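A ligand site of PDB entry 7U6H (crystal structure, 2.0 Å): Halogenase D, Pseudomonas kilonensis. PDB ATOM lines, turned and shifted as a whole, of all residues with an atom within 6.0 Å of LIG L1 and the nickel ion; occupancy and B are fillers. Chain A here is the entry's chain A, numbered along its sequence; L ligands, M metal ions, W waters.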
ATOM      1  N   THR A 137     -26.589 -15.245  -2.973  1.00  0.00           N
ATOM      2  CA  THR A 137     -27.240 -16.552  -3.111  1.00  0.00           C
ATOM      3  C   THR A 137     -28.380 -16.656  -2.124  1.00  0.00           C
ATOM      4  O   THR A 137     -28.331 -16.100  -1.017  1.00  0.00           O
ATOM      5  CB  THR A 137     -26.264 -17.726  -2.884  1.00  0.00           C
ATOM      6  OG1 THR A 137     -26.213 -18.041  -1.485  1.00  0.00           O
ATOM      7  CG2 THR A 137     -24.863 -17.389  -3.379  1.00  0.00           C
ATOM      8  N   LEU A 139     -30.904 -19.804  -0.653  1.00  0.00           N
ATOM      9  CA  LEU A 139     -31.346 -21.193  -0.583  1.00  0.00           C
ATOM     10  C   LEU A 139     -32.691 -21.241   0.141  1.00  0.00           C
ATOM     11  O   LEU A 139     -32.856 -20.623   1.188  1.00  0.00           O
ATOM     12  CB  LEU A 139     -30.321 -22.058   0.165  1.00  0.00           C
ATOM     13  CG  LEU A 139     -28.838 -21.884  -0.184  1.00  0.00           C
ATOM     14  CD1 LEU A 139     -27.986 -22.804   0.675  1.00  0.00           C
ATOM     15  CD2 LEU A 139     -28.584 -22.133  -1.654  1.00  0.00           C
ATOM     16  N   HIS A 146     -24.950 -25.452  -1.907  1.00  0.00           N
ATOM     17  CA  HIS A 146     -23.772 -24.853  -2.528  1.00  0.00           C
ATOM     18  C   HIS A 146     -22.661 -25.876  -2.312  1.00  0.00           C
ATOM     19  O   HIS A 146     -21.997 -25.867  -1.263  1.00  0.00           O
ATOM     20  CB  HIS A 146     -23.445 -23.490  -1.929  1.00  0.00           C
ATOM     21  CG  HIS A 146     -22.523 -22.664  -2.766  1.00  0.00           C
ATOM     22  ND1 HIS A 146     -22.586 -21.290  -2.816  1.00  0.00           N
ATOM     23  CD2 HIS A 146     -21.499 -23.020  -3.586  1.00  0.00           C
ATOM     24  CE1 HIS A 146     -21.655 -20.835  -3.625  1.00  0.00           C
ATOM     25  NE2 HIS A 146     -20.980 -21.867  -4.109  1.00  0.00           N
ATOM     26  N   HIS A 149     -16.427 -26.714  -2.999  1.00  0.00           N
ATOM     27  CA  HIS A 149     -15.743 -25.871  -3.965  1.00  0.00           C
ATOM     28  C   HIS A 149     -14.647 -25.093  -3.249  1.00  0.00           C
ATOM     29  O   HIS A 149     -14.542 -25.097  -2.027  1.00  0.00           O
ATOM     30  CB  HIS A 149     -16.711 -24.902  -4.646  1.00  0.00           C
ATOM     31  CG  HIS A 149     -17.255 -23.849  -3.726  1.00  0.00           C
ATOM     32  ND1 HIS A 149     -18.333 -24.061  -2.903  1.00  0.00           N
ATOM     33  CD2 HIS A 149     -16.854 -22.570  -3.502  1.00  0.00           C
ATOM     34  CE1 HIS A 149     -18.583 -22.961  -2.213  1.00  0.00           C
ATOM     35  NE2 HIS A 149     -17.696 -22.044  -2.554  1.00  0.00           N
ATOM     36  N   TRP A 150     -13.821 -24.423  -4.059  1.00  0.00           N
ATOM     37  CA  TRP A 150     -12.905 -23.388  -3.611  1.00  0.00           C
ATOM     38  C   TRP A 150     -13.258 -22.086  -4.331  1.00  0.00           C
ATOM     39  O   TRP A 150     -14.108 -22.052  -5.217  1.00  0.00           O
ATOM     40  CB  TRP A 150     -11.437 -23.745  -3.919  1.00  0.00           C
ATOM     41  CG  TRP A 150     -10.890 -24.932  -3.203  1.00  0.00           C
ATOM     42  CD1 TRP A 150     -10.144 -24.920  -2.052  1.00  0.00           C
ATOM     43  CD2 TRP A 150     -10.986 -26.306  -3.594  1.00  0.00           C
ATOM     44  NE1 TRP A 150      -9.795 -26.199  -1.704  1.00  0.00           N
ATOM     45  CE2 TRP A 150     -10.300 -27.070  -2.638  1.00  0.00           C
ATOM     46  CE3 TRP A 150     -11.602 -26.964  -4.674  1.00  0.00           C
ATOM     47  CZ2 TRP A 150     -10.206 -28.459  -2.710  1.00  0.00           C
ATOM     48  CZ3 TRP A 150     -11.507 -28.338  -4.743  1.00  0.00           C
ATOM     49  CH2 TRP A 150     -10.812 -29.069  -3.773  1.00  0.00           C
ATOM     50  N   GLY A 151     -12.588 -21.013  -3.929  1.00  0.00           N
ATOM     51  CA  GLY A 151     -12.683 -19.754  -4.624  1.00  0.00           C
ATOM     52  C   GLY A 151     -11.441 -19.502  -5.474  1.00  0.00           C
ATOM     53  O   GLY A 151     -10.347 -19.962  -5.152  1.00  0.00           O
ATOM     54  N   THR A 156     -12.551 -13.713   1.003  1.00  0.00           N
ATOM     55  CA  THR A 156     -13.989 -13.683   0.809  1.00  0.00           C
ATOM     56  C   THR A 156     -14.668 -13.332   2.125  1.00  0.00           C
ATOM     57  O   THR A 156     -14.319 -13.889   3.179  1.00  0.00           O
ATOM     58  CB  THR A 156     -14.495 -15.032   0.295  1.00  0.00           C
ATOM     59  OG1 THR A 156     -14.060 -15.225  -1.053  1.00  0.00           O
ATOM     60  CG2 THR A 156     -16.018 -15.095   0.343  1.00  0.00           C
ATOM     61  N   ILE A 158     -18.473 -13.338   3.790  1.00  0.00           N
ATOM     62  CA  ILE A 158     -19.817 -13.862   3.636  1.00  0.00           C
ATOM     63  C   ILE A 158     -20.712 -13.170   4.659  1.00  0.00           C
ATOM     64  O   ILE A 158     -20.497 -13.287   5.872  1.00  0.00           O
ATOM     65  CB  ILE A 158     -19.868 -15.384   3.793  1.00  0.00           C
ATOM     66  CG1 ILE A 158     -18.982 -16.060   2.757  1.00  0.00           C
ATOM     67  CG2 ILE A 158     -21.307 -15.888   3.691  1.00  0.00           C
ATOM     68  CD1 ILE A 158     -19.444 -15.829   1.324  1.00  0.00           C
ATOM     69  N   ILE A 160     -24.249 -12.919   6.324  1.00  0.00           N
ATOM     70  CA  ILE A 160     -25.455 -13.714   6.554  1.00  0.00           C
ATOM     71  C   ILE A 160     -26.635 -12.750   6.631  1.00  0.00           C
ATOM     72  O   ILE A 160     -26.791 -12.019   7.611  1.00  0.00           O
ATOM     73  CB  ILE A 160     -25.343 -14.572   7.813  1.00  0.00           C
ATOM     74  CG1 ILE A 160     -24.016 -15.329   7.823  1.00  0.00           C
ATOM     75  CG2 ILE A 160     -26.521 -15.530   7.915  1.00  0.00           C
ATOM     76  CD1 ILE A 160     -23.873 -16.337   6.706  1.00  0.00           C
ATOM     77  N   GLY A 171     -28.075 -25.698   5.779  1.00  0.00           N
ATOM     78  CA  GLY A 171     -27.295 -24.498   5.587  1.00  0.00           C
ATOM     79  C   GLY A 171     -26.012 -24.426   6.383  1.00  0.00           C
ATOM     80  O   GLY A 171     -25.377 -23.365   6.411  1.00  0.00           O
ATOM     81  N   LEU A 173     -22.199 -24.631   7.228  1.00  0.00           N
ATOM     82  CA  LEU A 173     -20.959 -24.524   6.468  1.00  0.00           C
ATOM     83  C   LEU A 173     -19.920 -25.480   7.035  1.00  0.00           C
ATOM     84  O   LEU A 173     -19.736 -25.550   8.261  1.00  0.00           O
ATOM     85  CB  LEU A 173     -20.426 -23.083   6.503  1.00  0.00           C
ATOM     86  CG  LEU A 173     -19.046 -22.867   5.884  1.00  0.00           C
ATOM     87  CD1 LEU A 173     -19.169 -22.619   4.379  1.00  0.00           C
ATOM     88  CD2 LEU A 173     -18.320 -21.715   6.565  1.00  0.00           C
ATOM     89  N   HIS A 202     -24.601 -20.279  11.186  1.00  0.00           N
ATOM     90  CA  HIS A 202     -24.623 -18.828  11.146  1.00  0.00           C
ATOM     91  C   HIS A 202     -26.050 -18.317  11.276  1.00  0.00           C
ATOM     92  O   HIS A 202     -27.008 -18.957  10.829  1.00  0.00           O
ATOM     93  CB  HIS A 202     -23.995 -18.298   9.844  1.00  0.00           C
ATOM     94  CG  HIS A 202     -22.599 -18.785   9.622  1.00  0.00           C
ATOM     95  ND1 HIS A 202     -22.320 -19.889   8.839  1.00  0.00           N
ATOM     96  CD2 HIS A 202     -21.417 -18.336  10.085  1.00  0.00           C
ATOM     97  CE1 HIS A 202     -21.007 -20.089   8.825  1.00  0.00           C
ATOM     98  NE2 HIS A 202     -20.444 -19.165   9.579  1.00  0.00           N
ATOM     99  N   TYR A 208     -18.665 -13.504   8.222  1.00  0.00           N
ATOM    100  CA  TYR A 208     -17.441 -14.254   8.477  1.00  0.00           C
ATOM    101  C   TYR A 208     -16.446 -14.094   7.341  1.00  0.00           C
ATOM    102  O   TYR A 208     -16.813 -13.933   6.171  1.00  0.00           O
ATOM    103  CB  TYR A 208     -17.733 -15.751   8.744  1.00  0.00           C
ATOM    104  CG  TYR A 208     -18.226 -16.591   7.594  1.00  0.00           C
ATOM    105  CD1 TYR A 208     -17.346 -17.126   6.655  1.00  0.00           C
ATOM    106  CD2 TYR A 208     -19.578 -16.911   7.468  1.00  0.00           C
ATOM    107  CE1 TYR A 208     -17.789 -17.915   5.619  1.00  0.00           C
ATOM    108  CE2 TYR A 208     -20.031 -17.700   6.431  1.00  0.00           C
ATOM    109  CZ  TYR A 208     -19.132 -18.202   5.507  1.00  0.00           C
ATOM    110  OH  TYR A 208     -19.575 -18.999   4.477  1.00  0.00           O
ATOM    111  N   LEU A 210     -13.406 -15.616   5.097  1.00  0.00           N
ATOM    112  CA  LEU A 210     -13.087 -16.942   4.583  1.00  0.00           C
ATOM    113  C   LEU A 210     -11.882 -16.857   3.663  1.00  0.00           C
ATOM    114  O   LEU A 210     -11.866 -16.038   2.735  1.00  0.00           O
ATOM    115  CB  LEU A 210     -14.287 -17.542   3.845  1.00  0.00           C
ATOM    116  CG  LEU A 210     -14.108 -18.916   3.207  1.00  0.00           C
ATOM    117  CD1 LEU A 210     -13.922 -19.990   4.268  1.00  0.00           C
ATOM    118  CD2 LEU A 210     -15.297 -19.245   2.316  1.00  0.00           C
ATOM    119  N   SER A 212     -10.808 -18.230   0.891  1.00  0.00           N
ATOM    120  CA  SER A 212     -11.614 -19.030  -0.031  1.00  0.00           C
ATOM    121  C   SER A 212     -10.778 -19.853  -1.004  1.00  0.00           C
ATOM    122  O   SER A 212     -11.257 -20.874  -1.500  1.00  0.00           O
ATOM    123  CB  SER A 212     -12.563 -18.122  -0.814  1.00  0.00           C
ATOM    124  OG  SER A 212     -11.941 -16.890  -1.140  1.00  0.00           O
ATOM    125  N   HIS A 217     -14.783 -25.867   0.965  1.00  0.00           N
ATOM    126  CA  HIS A 217     -15.970 -25.646   1.782  1.00  0.00           C
ATOM    127  C   HIS A 217     -17.224 -25.866   0.969  1.00  0.00           C
ATOM    128  O   HIS A 217     -17.200 -25.927  -0.259  1.00  0.00           O
ATOM    129  CB  HIS A 217     -15.973 -24.230   2.380  1.00  0.00           C
ATOM    130  CG  HIS A 217     -15.931 -23.135   1.359  1.00  0.00           C
ATOM    131  ND1 HIS A 217     -14.792 -22.829   0.646  1.00  0.00           N
ATOM    132  CD2 HIS A 217     -16.886 -22.270   0.936  1.00  0.00           C
ATOM    133  CE1 HIS A 217     -15.052 -21.826  -0.175  1.00  0.00           C
ATOM    134  NE2 HIS A 217     -16.314 -21.471  -0.020  1.00  0.00           N
ATOM    135  N   HIS A 218     -18.341 -26.015   1.684  1.00  0.00           N
ATOM    136  CA  HIS A 218     -19.643 -26.205   1.067  1.00  0.00           C
ATOM    137  C   HIS A 218     -20.716 -25.849   2.092  1.00  0.00           C
ATOM    138  O   HIS A 218     -20.446 -25.735   3.294  1.00  0.00           O
ATOM    139  CB  HIS A 218     -19.830 -27.636   0.563  1.00  0.00           C
ATOM    140  CG  HIS A 218     -20.273 -28.603   1.610  1.00  0.00           C
ATOM    141  ND1 HIS A 218     -21.384 -29.405   1.473  1.00  0.00           N
ATOM    142  CD2 HIS A 218     -19.742 -28.909   2.820  1.00  0.00           C
ATOM    143  CE1 HIS A 218     -21.524 -30.163   2.544  1.00  0.00           C
ATOM    144  NE2 HIS A 218     -20.541 -29.874   3.385  1.00  0.00           N
ATOM    145  N   VAL A 219     -21.942 -25.675   1.605  1.00  0.00           N
ATOM    146  CA  VAL A 219     -23.110 -25.421   2.437  1.00  0.00           C
ATOM    147  C   VAL A 219     -23.972 -26.676   2.417  1.00  0.00           C
ATOM    148  O   VAL A 219     -24.403 -27.114   1.344  1.00  0.00           O
ATOM    149  CB  VAL A 219     -23.889 -24.187   1.952  1.00  0.00           C
ATOM    150  CG1 VAL A 219     -25.131 -23.986   2.803  1.00  0.00           C
ATOM    151  CG2 VAL A 219     -23.009 -22.955   1.977  1.00  0.00           C
ATOM    152  N   ARG A 228     -32.411 -18.886   3.395  1.00  0.00           N
ATOM    153  CA  ARG A 228     -31.010 -18.652   3.720  1.00  0.00           C
ATOM    154  C   ARG A 228     -30.424 -17.759   2.638  1.00  0.00           C
ATOM    155  O   ARG A 228     -30.305 -18.178   1.485  1.00  0.00           O
ATOM    156  CB  ARG A 228     -30.228 -19.957   3.839  1.00  0.00           C
ATOM    157  CG  ARG A 228     -28.844 -19.786   4.439  1.00  0.00           C
ATOM    158  CD  ARG A 228     -27.983 -21.026   4.274  1.00  0.00           C
ATOM    159  NE  ARG A 228     -26.685 -20.877   4.920  1.00  0.00           N
ATOM    160  CZ  ARG A 228     -25.601 -20.395   4.312  1.00  0.00           C
ATOM    161  NH1 ARG A 228     -25.673 -20.010   3.045  1.00  0.00           N
ATOM    162  NH2 ARG A 228     -24.466 -20.291   4.976  1.00  0.00           N
ATOM    163  N   ILE A 230     -27.260 -14.992   1.631  1.00  0.00           N
ATOM    164  CA  ILE A 230     -25.922 -14.504   1.944  1.00  0.00           C
ATOM    165  C   ILE A 230     -25.464 -13.558   0.852  1.00  0.00           C
ATOM    166  O   ILE A 230     -25.900 -13.636  -0.302  1.00  0.00           O
ATOM    167  CB  ILE A 230     -24.910 -15.661   2.112  1.00  0.00           C
ATOM    168  CG1 ILE A 230     -24.713 -16.419   0.799  1.00  0.00           C
ATOM    169  CG2 ILE A 230     -25.339 -16.605   3.230  1.00  0.00           C
ATOM    170  CD1 ILE A 230     -23.403 -16.114   0.088  1.00  0.00           C
ATOM    171  N   ASN A 232     -21.779 -12.414  -0.861  1.00  0.00           N
ATOM    172  CA  ASN A 232     -20.379 -12.802  -0.994  1.00  0.00           C
ATOM    173  C   ASN A 232     -19.630 -11.626  -1.612  1.00  0.00           C
ATOM    174  O   ASN A 232     -19.854 -11.288  -2.772  1.00  0.00           O
ATOM    175  CB  ASN A 232     -20.237 -14.057  -1.852  1.00  0.00           C
ATOM    176  CG  ASN A 232     -18.785 -14.511  -2.021  1.00  0.00           C
ATOM    177  OD1 ASN A 232     -17.858 -13.705  -2.060  1.00  0.00           O
ATOM    178  ND2 ASN A 232     -18.594 -15.822  -2.127  1.00  0.00           N
ATOM    179  N   TRP A 254     -23.612 -17.801 -11.815  1.00  0.00           N
ATOM    180  CA  TRP A 254     -24.127 -16.441 -11.768  1.00  0.00           C
ATOM    181  C   TRP A 254     -24.183 -15.745 -13.129  1.00  0.00           C
ATOM    182  O   TRP A 254     -24.950 -14.788 -13.272  1.00  0.00           O
ATOM    183  CB  TRP A 254     -23.292 -15.581 -10.825  1.00  0.00           C
ATOM    184  CG  TRP A 254     -23.476 -15.889  -9.375  1.00  0.00           C
ATOM    185  CD1 TRP A 254     -24.467 -15.417  -8.560  1.00  0.00           C
ATOM    186  CD2 TRP A 254     -22.658 -16.734  -8.572  1.00  0.00           C
ATOM    187  NE1 TRP A 254     -24.307 -15.918  -7.291  1.00  0.00           N
ATOM    188  CE2 TRP A 254     -23.203 -16.734  -7.269  1.00  0.00           C
ATOM    189  CE3 TRP A 254     -21.508 -17.504  -8.812  1.00  0.00           C
ATOM    190  CZ2 TRP A 254     -22.646 -17.463  -6.225  1.00  0.00           C
ATOM    191  CZ3 TRP A 254     -20.960 -18.224  -7.774  1.00  0.00           C
ATOM    192  CH2 TRP A 254     -21.533 -18.198  -6.491  1.00  0.00           C
HETATM  193  C1  LIG L   1     -19.709 -18.664  -1.776  1.00  0.00           C
HETATM  194  O1  LIG L   1     -20.487 -17.709  -2.029  1.00  0.00           O
HETATM  195  O2  LIG L   1     -18.672 -18.827  -2.474  1.00  0.00           O
HETATM  196  C2  LIG L   1     -20.011 -19.608  -0.624  1.00  0.00           C
HETATM  197  O3  LIG L   1     -19.273 -20.493  -0.362  1.00  0.00           O
HETATM  198  C3  LIG L   1     -21.282 -19.412   0.216  1.00  0.00           C
HETATM  199  C4  LIG L   1     -20.943 -19.633   1.682  1.00  0.00           C
HETATM  200  C5  LIG L   1     -22.207 -19.545   2.525  1.00  0.00           C
HETATM  201  O4  LIG L   1     -23.339 -19.539   1.967  1.00  0.00           O
HETATM  202  O5  LIG L   1     -22.123 -19.489   3.778  1.00  0.00           O
HETATM  203 CL1  LG2 L   2     -15.487 -19.541  -2.655  1.00  0.00          CL
HETATM  204  N1  LG3 L   3     -15.888 -20.752  -7.319  1.00  0.00           N
HETATM  205  C1  LG3 L   3     -17.020 -20.786  -6.405  1.00  0.00           C
HETATM  206  C2  LG3 L   3     -17.756 -19.451  -6.370  1.00  0.00           C
HETATM  207  C3  LG3 L   3     -16.981 -18.404  -5.588  1.00  0.00           C
HETATM  208  C4  LG3 L   3     -17.643 -17.038  -5.691  1.00  0.00           C
HETATM  209  N2  LG3 L   3     -16.880 -15.912  -5.185  1.00  0.00           N
HETATM  210  C5  LG3 L   3     -18.059 -21.904  -6.743  1.00  0.00           C
HETATM  211  O1  LG3 L   3     -19.179 -21.859  -6.152  1.00  0.00           O
HETATM  212  O2  LG3 L   3     -17.730 -22.792  -7.575  1.00  0.00           O
HETATM  213 NI    NI M   1     -17.390 -20.343  -1.434  1.00  0.00          NI
HETATM  214  O   HOH W   1     -24.446 -19.733  -0.724  1.00  0.00           O
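The nickel ion is bound by NE2 of His 149 (2.1 Å), NE2 of His 217 (2.1 Å), O3 of LIG L1 (2.2 Å), O2 of LIG L1 (2.2 Å) and CL1 of LG2 L2 (2.4 Å).
The nickel ion has five donor atoms within binding distance.
An oxygen (O1) of LIG L1 is in hydrogen-bond range of the side-chain amide nitrogen (ND2) of Asn 232, at 2.7 Å.
NE2 of His 146 sits at hydrogen-bond distance from O1 of LG3 L3 (2.7 Å).
An oxygen (O5) of LIG L1 lies within hydrogen-bond range of the side-chain hydroxyl (OH) of Tyr 208, at 2.7 Å.
O of Trp 150 is in hydrogen-bond range of N1 of LG3 L3 (3.0 Å).
An oxygen (O4) of LIG L1 is in salt-bridge range of the guanidinium group (NH1) of Arg 228 (2.6 Å).
Of the 22 residues printed, 2 come within 4 Å of the nickel ion.
The nearest printed residue that does not touch the nickel ion is Leu 210 (4.4 Å).
O of Arg 228 is in hydrogen-bond range of N of Leu 139.
O of Tyr 208 is in hydrogen-bond range of N of Ile 158.
The backbone NH (N) of Val 219 sits at hydrogen-bond distance from the backbone carbonyl oxygen (O) of His 146.
NE of Arg 228 sits at hydrogen-bond distance from O of Gly 171 (3.2 Å).
The backbone NH (N) of Ile 230 is in hydrogen-bond range of the backbone carbonyl oxygen (O) of Thr 137, 3.1 Å away.
Water W1 lies within hydrogen-bond range of the side-chain hydroxyl (OG1) of Thr 137 (2.6 Å), an oxygen (O4) of LIG L1 (2.9 Å) and a ring nitrogen (ND1) of His 146 (3.2 Å).
Residues that only touch LIG L1: Val 219, His 146, Ile 230 and Ile 158.
Hydrophobic or aromatic side chains within 4 Å of LIG L1: His 146, His 149, Ile 158, Tyr 208, His 217, Val 219 and Ile 230.
Nine residues have an atom within 4 Å of LIG L1: His 146, His 149, Ile 158, Tyr 208, His 217, Val 219, Arg 228, Ile 230 and Asn 232.
The nearest printed residue that does not touch LIG L1 is Leu 173 (4.3 Å).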
